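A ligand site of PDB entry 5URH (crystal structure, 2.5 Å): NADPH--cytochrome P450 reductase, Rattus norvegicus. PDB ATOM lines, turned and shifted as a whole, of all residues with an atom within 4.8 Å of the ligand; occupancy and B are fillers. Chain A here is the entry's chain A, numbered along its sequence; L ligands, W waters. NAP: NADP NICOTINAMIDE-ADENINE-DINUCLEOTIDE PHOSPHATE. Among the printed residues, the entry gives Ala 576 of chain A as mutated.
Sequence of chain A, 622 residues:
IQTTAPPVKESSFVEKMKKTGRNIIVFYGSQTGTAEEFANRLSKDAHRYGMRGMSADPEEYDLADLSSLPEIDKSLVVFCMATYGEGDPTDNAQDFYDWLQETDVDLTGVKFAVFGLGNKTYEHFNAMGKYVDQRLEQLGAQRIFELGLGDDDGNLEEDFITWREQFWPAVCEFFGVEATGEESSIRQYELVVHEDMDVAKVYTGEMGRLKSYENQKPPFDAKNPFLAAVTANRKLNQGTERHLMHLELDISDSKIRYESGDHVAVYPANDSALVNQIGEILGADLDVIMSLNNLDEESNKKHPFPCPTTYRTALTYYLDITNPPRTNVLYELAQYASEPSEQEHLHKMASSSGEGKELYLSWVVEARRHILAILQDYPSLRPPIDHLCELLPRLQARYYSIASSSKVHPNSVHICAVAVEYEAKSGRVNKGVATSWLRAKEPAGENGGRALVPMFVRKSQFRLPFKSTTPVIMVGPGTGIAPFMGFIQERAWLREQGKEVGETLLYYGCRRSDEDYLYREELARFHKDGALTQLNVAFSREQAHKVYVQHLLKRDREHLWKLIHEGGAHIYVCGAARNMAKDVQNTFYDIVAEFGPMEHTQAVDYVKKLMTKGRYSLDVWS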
ATOM      1  N   ARG A 242     -24.576  27.329 -18.784  1.00  0.00           N
ATOM      2  CA  ARG A 242     -23.534  28.332 -19.012  1.00  0.00           C
ATOM      3  C   ARG A 242     -22.799  28.000 -20.302  1.00  0.00           C
ATOM      4  O   ARG A 242     -23.140  27.043 -20.996  1.00  0.00           O
ATOM      5  CB  ARG A 242     -22.524  28.340 -17.855  1.00  0.00           C
ATOM      6  CG  ARG A 242     -23.143  28.285 -16.483  1.00  0.00           C
ATOM      7  CD  ARG A 242     -22.437  27.234 -15.663  1.00  0.00           C
ATOM      8  NE  ARG A 242     -21.218  27.756 -15.073  1.00  0.00           N
ATOM      9  CZ  ARG A 242     -20.207  27.003 -14.666  1.00  0.00           C
ATOM     10  NH1 ARG A 242     -20.248  25.685 -14.772  1.00  0.00           N
ATOM     11  NH2 ARG A 242     -19.145  27.585 -14.116  1.00  0.00           N
ATOM     12  N   LEU A 244     -19.040  27.139 -21.678  1.00  0.00           N
ATOM     13  CA  LEU A 244     -17.627  26.888 -21.453  1.00  0.00           C
ATOM     14  C   LEU A 244     -17.026  26.607 -22.809  1.00  0.00           C
ATOM     15  O   LEU A 244     -17.566  25.794 -23.571  1.00  0.00           O
ATOM     16  CB  LEU A 244     -17.436  25.736 -20.470  1.00  0.00           C
ATOM     17  CG  LEU A 244     -17.851  26.202 -19.073  1.00  0.00           C
ATOM     18  CD1 LEU A 244     -19.322  25.874 -18.893  1.00  0.00           C
ATOM     19  CD2 LEU A 244     -16.999  25.568 -17.978  1.00  0.00           C
ATOM     20  N   VAL A 418     -14.630  29.917 -19.100  1.00  0.00           N
ATOM     21  CA  VAL A 418     -16.056  30.029 -18.935  1.00  0.00           C
ATOM     22  C   VAL A 418     -16.471  31.474 -19.214  1.00  0.00           C
ATOM     23  O   VAL A 418     -15.956  32.416 -18.608  1.00  0.00           O
ATOM     24  CB  VAL A 418     -16.505  29.613 -17.521  1.00  0.00           C
ATOM     25  CG1 VAL A 418     -15.745  30.398 -16.466  1.00  0.00           C
ATOM     26  CG2 VAL A 418     -18.010  29.830 -17.384  1.00  0.00           C
ATOM     27  N   PRO A 477     -11.014  21.683  -9.837  1.00  0.00           N
ATOM     28  CA  PRO A 477     -12.444  21.703 -10.177  1.00  0.00           C
ATOM     29  C   PRO A 477     -12.791  22.706 -11.284  1.00  0.00           C
ATOM     30  O   PRO A 477     -12.096  23.715 -11.494  1.00  0.00           O
ATOM     31  CB  PRO A 477     -13.099  22.056  -8.839  1.00  0.00           C
ATOM     32  CG  PRO A 477     -12.094  22.933  -8.207  1.00  0.00           C
ATOM     33  CD  PRO A 477     -10.784  22.217  -8.498  1.00  0.00           C
ATOM     34  N   GLY A 478     -13.878  22.403 -12.004  1.00  0.00           N
ATOM     35  CA  GLY A 478     -14.344  23.263 -13.077  1.00  0.00           C
ATOM     36  C   GLY A 478     -13.274  23.622 -14.094  1.00  0.00           C
ATOM     37  O   GLY A 478     -12.514  22.759 -14.557  1.00  0.00           O
ATOM     38  N   THR A 479     -13.222  24.898 -14.451  1.00  0.00           N
ATOM     39  CA  THR A 479     -12.241  25.376 -15.407  1.00  0.00           C
ATOM     40  C   THR A 479     -10.832  25.246 -14.838  1.00  0.00           C
ATOM     41  O   THR A 479      -9.858  25.514 -15.533  1.00  0.00           O
ATOM     42  CB  THR A 479     -12.470  26.856 -15.734  1.00  0.00           C
ATOM     43  OG1 THR A 479     -12.379  27.622 -14.522  1.00  0.00           O
ATOM     44  CG2 THR A 479     -13.856  27.064 -16.358  1.00  0.00           C
ATOM     45  N   GLY A 480     -10.724  24.829 -13.585  1.00  0.00           N
ATOM     46  CA  GLY A 480      -9.405  24.691 -12.997  1.00  0.00           C
ATOM     47  C   GLY A 480      -8.630  23.539 -13.590  1.00  0.00           C
ATOM     48  O   GLY A 480      -7.498  23.294 -13.218  1.00  0.00           O
ATOM     49  N   GLY A 509     -13.769  18.155 -10.765  1.00  0.00           N
ATOM     50  CA  GLY A 509     -15.140  18.316 -10.297  1.00  0.00           C
ATOM     51  C   GLY A 509     -15.981  19.169 -11.213  1.00  0.00           C
ATOM     52  O   GLY A 509     -15.497  20.126 -11.807  1.00  0.00           O
ATOM     53  N   CYS A 510     -17.247  18.813 -11.353  1.00  0.00           N
ATOM     54  CA  CYS A 510     -18.166  19.578 -12.171  1.00  0.00           C
ATOM     55  C   CYS A 510     -19.523  19.407 -11.491  1.00  0.00           C
ATOM     56  O   CYS A 510     -19.618  18.740 -10.473  1.00  0.00           O
ATOM     57  CB  CYS A 510     -18.167  19.075 -13.613  1.00  0.00           C
ATOM     58  SG  CYS A 510     -18.864  17.447 -13.887  1.00  0.00           S
ATOM     59  N   ARG A 511     -20.556  20.023 -12.045  1.00  0.00           N
ATOM     60  CA  ARG A 511     -21.883  19.934 -11.448  1.00  0.00           C
ATOM     61  C   ARG A 511     -22.609  18.640 -11.803  1.00  0.00           C
ATOM     62  O   ARG A 511     -23.114  17.961 -10.912  1.00  0.00           O
ATOM     63  CB  ARG A 511     -22.720  21.137 -11.879  1.00  0.00           C
ATOM     64  CG  ARG A 511     -21.988  22.429 -11.686  1.00  0.00           C
ATOM     65  CD  ARG A 511     -22.825  23.650 -11.988  1.00  0.00           C
ATOM     66  NE  ARG A 511     -22.030  24.854 -11.747  1.00  0.00           N
ATOM     67  CZ  ARG A 511     -22.490  26.095 -11.825  1.00  0.00           C
ATOM     68  NH1 ARG A 511     -23.760  26.328 -12.141  1.00  0.00           N
ATOM     69  NH2 ARG A 511     -21.673  27.110 -11.593  1.00  0.00           N
ATOM     70  N   ASP A 516     -21.802  20.083 -17.478  1.00  0.00           N
ATOM     71  CA  ASP A 516     -20.535  20.745 -17.735  1.00  0.00           C
ATOM     72  C   ASP A 516     -19.285  19.912 -17.438  1.00  0.00           C
ATOM     73  O   ASP A 516     -18.333  20.419 -16.856  1.00  0.00           O
ATOM     74  CB  ASP A 516     -20.469  22.055 -16.957  1.00  0.00           C
ATOM     75  CG  ASP A 516     -20.801  21.884 -15.488  1.00  0.00           C
ATOM     76  OD1 ASP A 516     -20.715  20.738 -14.992  1.00  0.00           O
ATOM     77  OD2 ASP A 516     -21.135  22.892 -14.828  1.00  0.00           O
ATOM     78  N   ALA A 538     -15.819  14.418  -9.180  1.00  0.00           N
ATOM     79  CA  ALA A 538     -16.838  14.732  -8.199  1.00  0.00           C
ATOM     80  C   ALA A 538     -17.960  15.518  -8.876  1.00  0.00           C
ATOM     81  O   ALA A 538     -17.732  16.623  -9.375  1.00  0.00           O
ATOM     82  CB  ALA A 538     -16.253  15.545  -7.061  1.00  0.00           C
ATOM     83  N   SER A 540     -20.796  17.587  -8.179  1.00  0.00           N
ATOM     84  CA  SER A 540     -21.363  18.296  -7.059  1.00  0.00           C
ATOM     85  C   SER A 540     -22.880  18.341  -6.974  1.00  0.00           C
ATOM     86  O   SER A 540     -23.411  18.494  -5.886  1.00  0.00           O
ATOM     87  CB  SER A 540     -20.812  19.715  -6.976  1.00  0.00           C
ATOM     88  OG  SER A 540     -21.214  20.492  -8.075  1.00  0.00           O
ATOM     89  N   ARG A 541     -23.578  18.175  -8.100  1.00  0.00           N
ATOM     90  CA  ARG A 541     -25.033  18.255  -8.038  1.00  0.00           C
ATOM     91  C   ARG A 541     -25.818  17.055  -8.534  1.00  0.00           C
ATOM     92  O   ARG A 541     -26.992  17.194  -8.890  1.00  0.00           O
ATOM     93  CB  ARG A 541     -25.520  19.501  -8.797  1.00  0.00           C
ATOM     94  CG  ARG A 541     -24.714  20.748  -8.442  1.00  0.00           C
ATOM     95  CD  ARG A 541     -25.316  21.999  -9.010  1.00  0.00           C
ATOM     96  NE  ARG A 541     -24.483  23.153  -8.677  1.00  0.00           N
ATOM     97  CZ  ARG A 541     -24.747  24.385  -9.082  1.00  0.00           C
ATOM     98  NH1 ARG A 541     -25.816  24.628  -9.837  1.00  0.00           N
ATOM     99  NH2 ARG A 541     -23.928  25.385  -8.763  1.00  0.00           N
ATOM    100  N   LYS A 546     -23.495  17.749  -1.506  1.00  0.00           N
ATOM    101  CA  LYS A 546     -22.400  18.140  -2.385  1.00  0.00           C
ATOM    102  C   LYS A 546     -21.309  17.089  -2.351  1.00  0.00           C
ATOM    103  O   LYS A 546     -21.048  16.476  -1.324  1.00  0.00           O
ATOM    104  CB  LYS A 546     -21.799  19.460  -1.926  1.00  0.00           C
ATOM    105  CG  LYS A 546     -22.704  20.667  -2.020  1.00  0.00           C
ATOM    106  CD  LYS A 546     -23.062  21.019  -3.455  1.00  0.00           C
ATOM    107  CE  LYS A 546     -23.721  22.385  -3.523  1.00  0.00           C
ATOM    108  NZ  LYS A 546     -24.166  22.755  -4.897  1.00  0.00           N
ATOM    109  N   TYR A 548     -17.470  17.138  -3.518  1.00  0.00           N
ATOM    110  CA  TYR A 548     -16.406  17.988  -4.023  1.00  0.00           C
ATOM    111  C   TYR A 548     -15.122  17.218  -4.166  1.00  0.00           C
ATOM    112  O   TYR A 548     -14.998  16.124  -3.614  1.00  0.00           O
ATOM    113  CB  TYR A 548     -16.192  19.173  -3.068  1.00  0.00           C
ATOM    114  CG  TYR A 548     -17.338  20.158  -3.031  1.00  0.00           C
ATOM    115  CD1 TYR A 548     -17.991  20.520  -4.204  1.00  0.00           C
ATOM    116  CD2 TYR A 548     -17.700  20.788  -1.853  1.00  0.00           C
ATOM    117  CE1 TYR A 548     -18.983  21.490  -4.217  1.00  0.00           C
ATOM    118  CE2 TYR A 548     -18.693  21.760  -1.844  1.00  0.00           C
ATOM    119  CZ  TYR A 548     -19.330  22.106  -3.036  1.00  0.00           C
ATOM    120  OH  TYR A 548     -20.303  23.095  -3.064  1.00  0.00           O
ATOM    121  N   VAL A 549     -14.151  17.782  -4.874  1.00  0.00           N
ATOM    122  CA  VAL A 549     -12.894  17.071  -5.037  1.00  0.00           C
ATOM    123  C   VAL A 549     -12.227  16.703  -3.706  1.00  0.00           C
ATOM    124  O   VAL A 549     -11.691  15.600  -3.578  1.00  0.00           O
ATOM    125  CB  VAL A 549     -11.900  17.857  -5.949  1.00  0.00           C
ATOM    126  CG1 VAL A 549     -12.517  18.015  -7.344  1.00  0.00           C
ATOM    127  CG2 VAL A 549     -11.573  19.225  -5.342  1.00  0.00           C
ATOM    128  N   GLN A 550     -12.285  17.588  -2.702  1.00  0.00           N
ATOM    129  CA  GLN A 550     -11.653  17.280  -1.423  1.00  0.00           C
ATOM    130  C   GLN A 550     -12.258  16.083  -0.715  1.00  0.00           C
ATOM    131  O   GLN A 550     -11.647  15.548   0.219  1.00  0.00           O
ATOM    132  CB  GLN A 550     -11.687  18.488  -0.465  1.00  0.00           C
ATOM    133  CG  GLN A 550     -13.055  19.075  -0.210  1.00  0.00           C
ATOM    134  CD  GLN A 550     -13.341  20.199  -1.164  1.00  0.00           C
ATOM    135  OE1 GLN A 550     -13.089  20.093  -2.364  1.00  0.00           O
ATOM    136  NE2 GLN A 550     -13.892  21.292  -0.631  1.00  0.00           N
ATOM    137  N   ALA A 576     -10.878  28.553  -9.450  1.00  0.00           N
ATOM    138  CA  ALA A 576     -11.415  29.828  -9.018  1.00  0.00           C
ATOM    139  C   ALA A 576     -11.348  30.024  -7.495  1.00  0.00           C
ATOM    140  O   ALA A 576     -11.718  29.129  -6.735  1.00  0.00           O
ATOM    141  CB  ALA A 576     -12.843  29.966  -9.494  1.00  0.00           C
ATOM    142  N   ASN A 579     -12.100  29.424  -0.531  1.00  0.00           N
ATOM    143  CA  ASN A 579     -12.798  28.213  -0.132  1.00  0.00           C
ATOM    144  C   ASN A 579     -12.127  26.963  -0.694  1.00  0.00           C
ATOM    145  O   ASN A 579     -11.413  26.254   0.018  1.00  0.00           O
ATOM    146  CB  ASN A 579     -14.262  28.270  -0.571  1.00  0.00           C
ATOM    147  CG  ASN A 579     -15.212  28.447   0.592  1.00  0.00           C
ATOM    148  OD1 ASN A 579     -15.513  29.575   0.990  1.00  0.00           O
ATOM    149  ND2 ASN A 579     -15.688  27.343   1.149  1.00  0.00           N
ATOM    150  N   MET A 580     -12.380  26.685  -1.977  1.00  0.00           N
ATOM    151  CA  MET A 580     -11.793  25.506  -2.640  1.00  0.00           C
ATOM    152  C   MET A 580     -10.321  25.243  -2.334  1.00  0.00           C
ATOM    153  O   MET A 580      -9.966  24.193  -1.802  1.00  0.00           O
ATOM    154  CB  MET A 580     -11.995  25.600  -4.147  1.00  0.00           C
ATOM    155  CG  MET A 580     -11.732  24.296  -4.932  1.00  0.00           C
ATOM    156  SD  MET A 580      -9.975  23.900  -5.229  1.00  0.00           S
ATOM    157  CE  MET A 580      -9.470  25.353  -6.109  1.00  0.00           C
ATOM    158  N   ASP A 583      -9.964  24.558   1.353  1.00  0.00           N
ATOM    159  CA  ASP A 583     -10.575  23.291   1.730  1.00  0.00           C
ATOM    160  C   ASP A 583      -9.691  22.121   1.319  1.00  0.00           C
ATOM    161  O   ASP A 583      -9.545  21.155   2.067  1.00  0.00           O
ATOM    162  CB  ASP A 583     -11.962  23.134   1.107  1.00  0.00           C
ATOM    163  CG  ASP A 583     -12.979  24.129   1.661  1.00  0.00           C
ATOM    164  OD1 ASP A 583     -12.785  24.607   2.797  1.00  0.00           O
ATOM    165  OD2 ASP A 583     -13.981  24.410   0.960  1.00  0.00           O
ATOM    166  N   SER A 622      -9.192  34.769  -8.708  1.00  0.00           N
ATOM    167  CA  SER A 622     -10.515  35.122  -8.219  1.00  0.00           C
ATOM    168  C   SER A 622     -11.578  34.912  -9.310  1.00  0.00           C
ATOM    169  O   SER A 622     -11.184  34.847 -10.503  1.00  0.00           O
ATOM    170  CB  SER A 622     -10.545  36.581  -7.747  1.00  0.00           C
ATOM    171  OG  SER A 622     -11.812  36.917  -7.185  1.00  0.00           O
ATOM    172  OXT SER A 622     -12.777  34.824  -8.968  1.00  0.00           O
HETATM  173  PA  NAP L   1     -17.818  26.003 -10.982  1.00  0.00           P
HETATM  174  O1A NAP L   1     -18.515  25.297 -12.081  1.00  0.00           O
HETATM  175  O2A NAP L   1     -18.496  27.126 -10.300  1.00  0.00           O
HETATM  176  O5B NAP L   1     -17.351  24.921  -9.883  1.00  0.00           O
HETATM  177  C5B NAP L   1     -16.737  23.704 -10.308  1.00  0.00           C
HETATM  178  C4B NAP L   1     -17.048  22.631  -9.263  1.00  0.00           C
HETATM  179  O4B NAP L   1     -16.464  23.079  -8.020  1.00  0.00           O
HETATM  180  C3B NAP L   1     -18.551  22.575  -9.042  1.00  0.00           C
HETATM  181  O3B NAP L   1     -18.970  21.204  -8.889  1.00  0.00           O
HETATM  182  C2B NAP L   1     -18.745  23.336  -7.746  1.00  0.00           C
HETATM  183  O2B NAP L   1     -19.881  22.781  -7.051  1.00  0.00           O
HETATM  184  C1B NAP L   1     -17.487  22.892  -7.030  1.00  0.00           C
HETATM  185  N9A NAP L   1     -17.187  23.683  -5.810  1.00  0.00           N
HETATM  186  C8A NAP L   1     -17.867  24.725  -5.364  1.00  0.00           C
HETATM  187  N7A NAP L   1     -17.349  25.073  -4.191  1.00  0.00           N
HETATM  188  C5A NAP L   1     -16.354  24.238  -3.911  1.00  0.00           C
HETATM  189  C6A NAP L   1     -15.632  24.081  -2.799  1.00  0.00           C
HETATM  190  N6A NAP L   1     -15.665  25.081  -1.925  1.00  0.00           N
HETATM  191  N1A NAP L   1     -14.749  23.081  -2.672  1.00  0.00           N
HETATM  192  C2A NAP L   1     -14.569  22.187  -3.741  1.00  0.00           C
HETATM  193  N3A NAP L   1     -15.338  22.390  -4.896  1.00  0.00           N
HETATM  194  C4A NAP L   1     -16.226  23.398  -4.934  1.00  0.00           C
HETATM  195  O3  NAP L   1     -16.387  26.524 -11.505  1.00  0.00           O
HETATM  196  PN  NAP L   1     -15.796  27.455 -12.666  1.00  0.00           P
HETATM  197  O1N NAP L   1     -16.545  27.167 -13.914  1.00  0.00           O
HETATM  198  O2N NAP L   1     -14.321  27.342 -12.684  1.00  0.00           O
HETATM  199  O5D NAP L   1     -16.195  28.928 -12.151  1.00  0.00           O
HETATM  200  C5D NAP L   1     -17.321  29.602 -12.728  1.00  0.00           C
HETATM  201  C4D NAP L   1     -17.569  30.942 -12.022  1.00  0.00           C
HETATM  202  O4D NAP L   1     -17.954  30.695 -10.661  1.00  0.00           O
HETATM  203  C3D NAP L   1     -16.281  31.751 -11.954  1.00  0.00           C
HETATM  204  O3D NAP L   1     -16.553  33.136 -12.189  1.00  0.00           O
HETATM  205  C2D NAP L   1     -15.852  31.541 -10.515  1.00  0.00           C
HETATM  206  O2D NAP L   1     -15.029  32.638 -10.083  1.00  0.00           O
HETATM  207  C1D NAP L   1     -17.219  31.640  -9.869  1.00  0.00           C
HETATM  208  N1N NAP L   1     -17.212  31.286  -8.434  1.00  0.00           N
HETATM  209  P2B NAP L   1     -21.221  23.624  -6.801  1.00  0.00           P
HETATM  210  O1X NAP L   1     -21.148  24.746  -7.754  1.00  0.00           O
HETATM  211  O2X NAP L   1     -21.123  24.023  -5.371  1.00  0.00           O
HETATM  212  O3X NAP L   1     -22.299  22.642  -7.076  1.00  0.00           O
HETATM  213  O   HOH W   1     -12.820  26.692 -10.408  1.00  0.00           O
HETATM  214  O   HOH W   2     -17.314  19.222  -7.787  1.00  0.00           O
HETATM  215  O   HOH W   3     -18.863  26.424  -1.855  1.00  0.00           O
HETATM  216  O   HOH W   4     -19.909  30.477 -14.122  1.00  0.00           O
HETATM  217  O   HOH W   5     -18.699  22.699 -12.901  1.00  0.00           O
HETATM  218  O   HOH W   6     -15.032  19.924  -6.504  1.00  0.00           O
HETATM  219  O   HOH W   7     -19.785  27.135  -8.010  1.00  0.00           O
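The chain-end carboxylate (OXT) of Ser 622 lies within hydrogen-bond range of an oxygen (O2D) of the ligand, at 3.3 Å.
An oxygen (O3B) of the ligand sits at hydrogen-bond distance from the side-chain hydroxyl (OG) of Ser 540, 2.5 Å away.
N of Thr 479 lies within hydrogen-bond range of O2N of the ligand (3.2 Å).
The side-chain carboxylate (OD2) of Asp 583 sits at hydrogen-bond distance from a nitrogen (N6A) of the ligand, 3.4 Å away.
NZ of Lys 546 lies within salt-bridge range of O3X of the ligand (2.9 Å).
N1A of the ligand is in hydrogen-bond range of NE2 of Gln 550.
The side-chain hydroxyl of Tyr 548 lies within hydrogen-bond range of an oxygen (O2X) of the ligand, 2.6 Å away.
NH2 of Arg 242 is in salt-bridge range of O1N of the ligand (2.6 Å).
The backbone carbonyl oxygen (O) of Cys 510 sits at hydrogen-bond distance from an oxygen (O3B) of the ligand (3.0 Å).
NE of Arg 541 is in salt-bridge range of O3X of the ligand.
OG1 of Thr 479 is in hydrogen-bond range of O2N of the ligand, at 2.7 Å.
NH2 of Arg 511 lies within salt-bridge range of O2A of the ligand (3.4 Å).
OD2 of Asp 583 is in hydrogen-bond range of ND2 of Asn 579.
The backbone NH (N) of Arg 541 is in hydrogen-bond range of the backbone carbonyl oxygen (O) of Arg 511, at 2.9 Å.
The backbone NH of Ser 540 lies within hydrogen-bond range of the backbone carbonyl oxygen of Cys 510 (2.8 Å).
N of Cys 510 is in hydrogen-bond range of O of Ala 538, at 3.0 Å.
The backbone carbonyl oxygen of Gly 509 lies within hydrogen-bond range of the backbone NH of Gly 478 (2.8 Å).
The guanidinium group of Arg 511 lies within salt-bridge range of the side-chain carboxylate of Asp 516, at 3.8 Å.
NH1 of Arg 242 lies within salt-bridge range of OD2 of Asp 516, at 2.9 Å.
Pro 477 touches the ligand (CB to O4B, 3.6 Å).
Gly 478 touches the ligand.
Gly 509 touches the ligand (O to C4B, 3.9 Å).
Ala 576 touches the ligand.
Asn 579 touches the ligand.
N of Met 580 touches N6A of the ligand, at 3.7 Å.
Hydrophobic or aromatic side chains that line the ligand: Pro 477, Tyr 548, Ala 576 and Met 580.
Within 4 Å of the ligand: Arg 242, Pro 477, Gly 478, Thr 479, Gly 509, Cys 510, Arg 511, Ser 540, Arg 541, Lys 546, Tyr 548, Gln 550, Ala 576, Asn 579, Met 580, Asp 583 and Ser 622.
Along chain A the residues within 4 Å of the ligand span positions 242 to 622.
The nearest printed residue that does not touch the ligand is Val 418 (4.1 Å).
Water W5 lies within hydrogen-bond range of an oxygen (O1A) of the ligand (2.7 Å), the side-chain carboxylate of Asp 516 (3.1 Å) and the backbone NH of Arg 511 (3.4 Å).
Water W1 lies within hydrogen-bond range of O2N of the ligand (2.8 Å), N of Ala 576 (2.9 Å) and O of Pro 477 (3.3 Å).
Water W2 bridges O3B of the ligand and O of Ala 538.
Water W6 lies within hydrogen-bond range of N of Val 549 (2.8 Å) and N3A of the ligand (3.0 Å).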
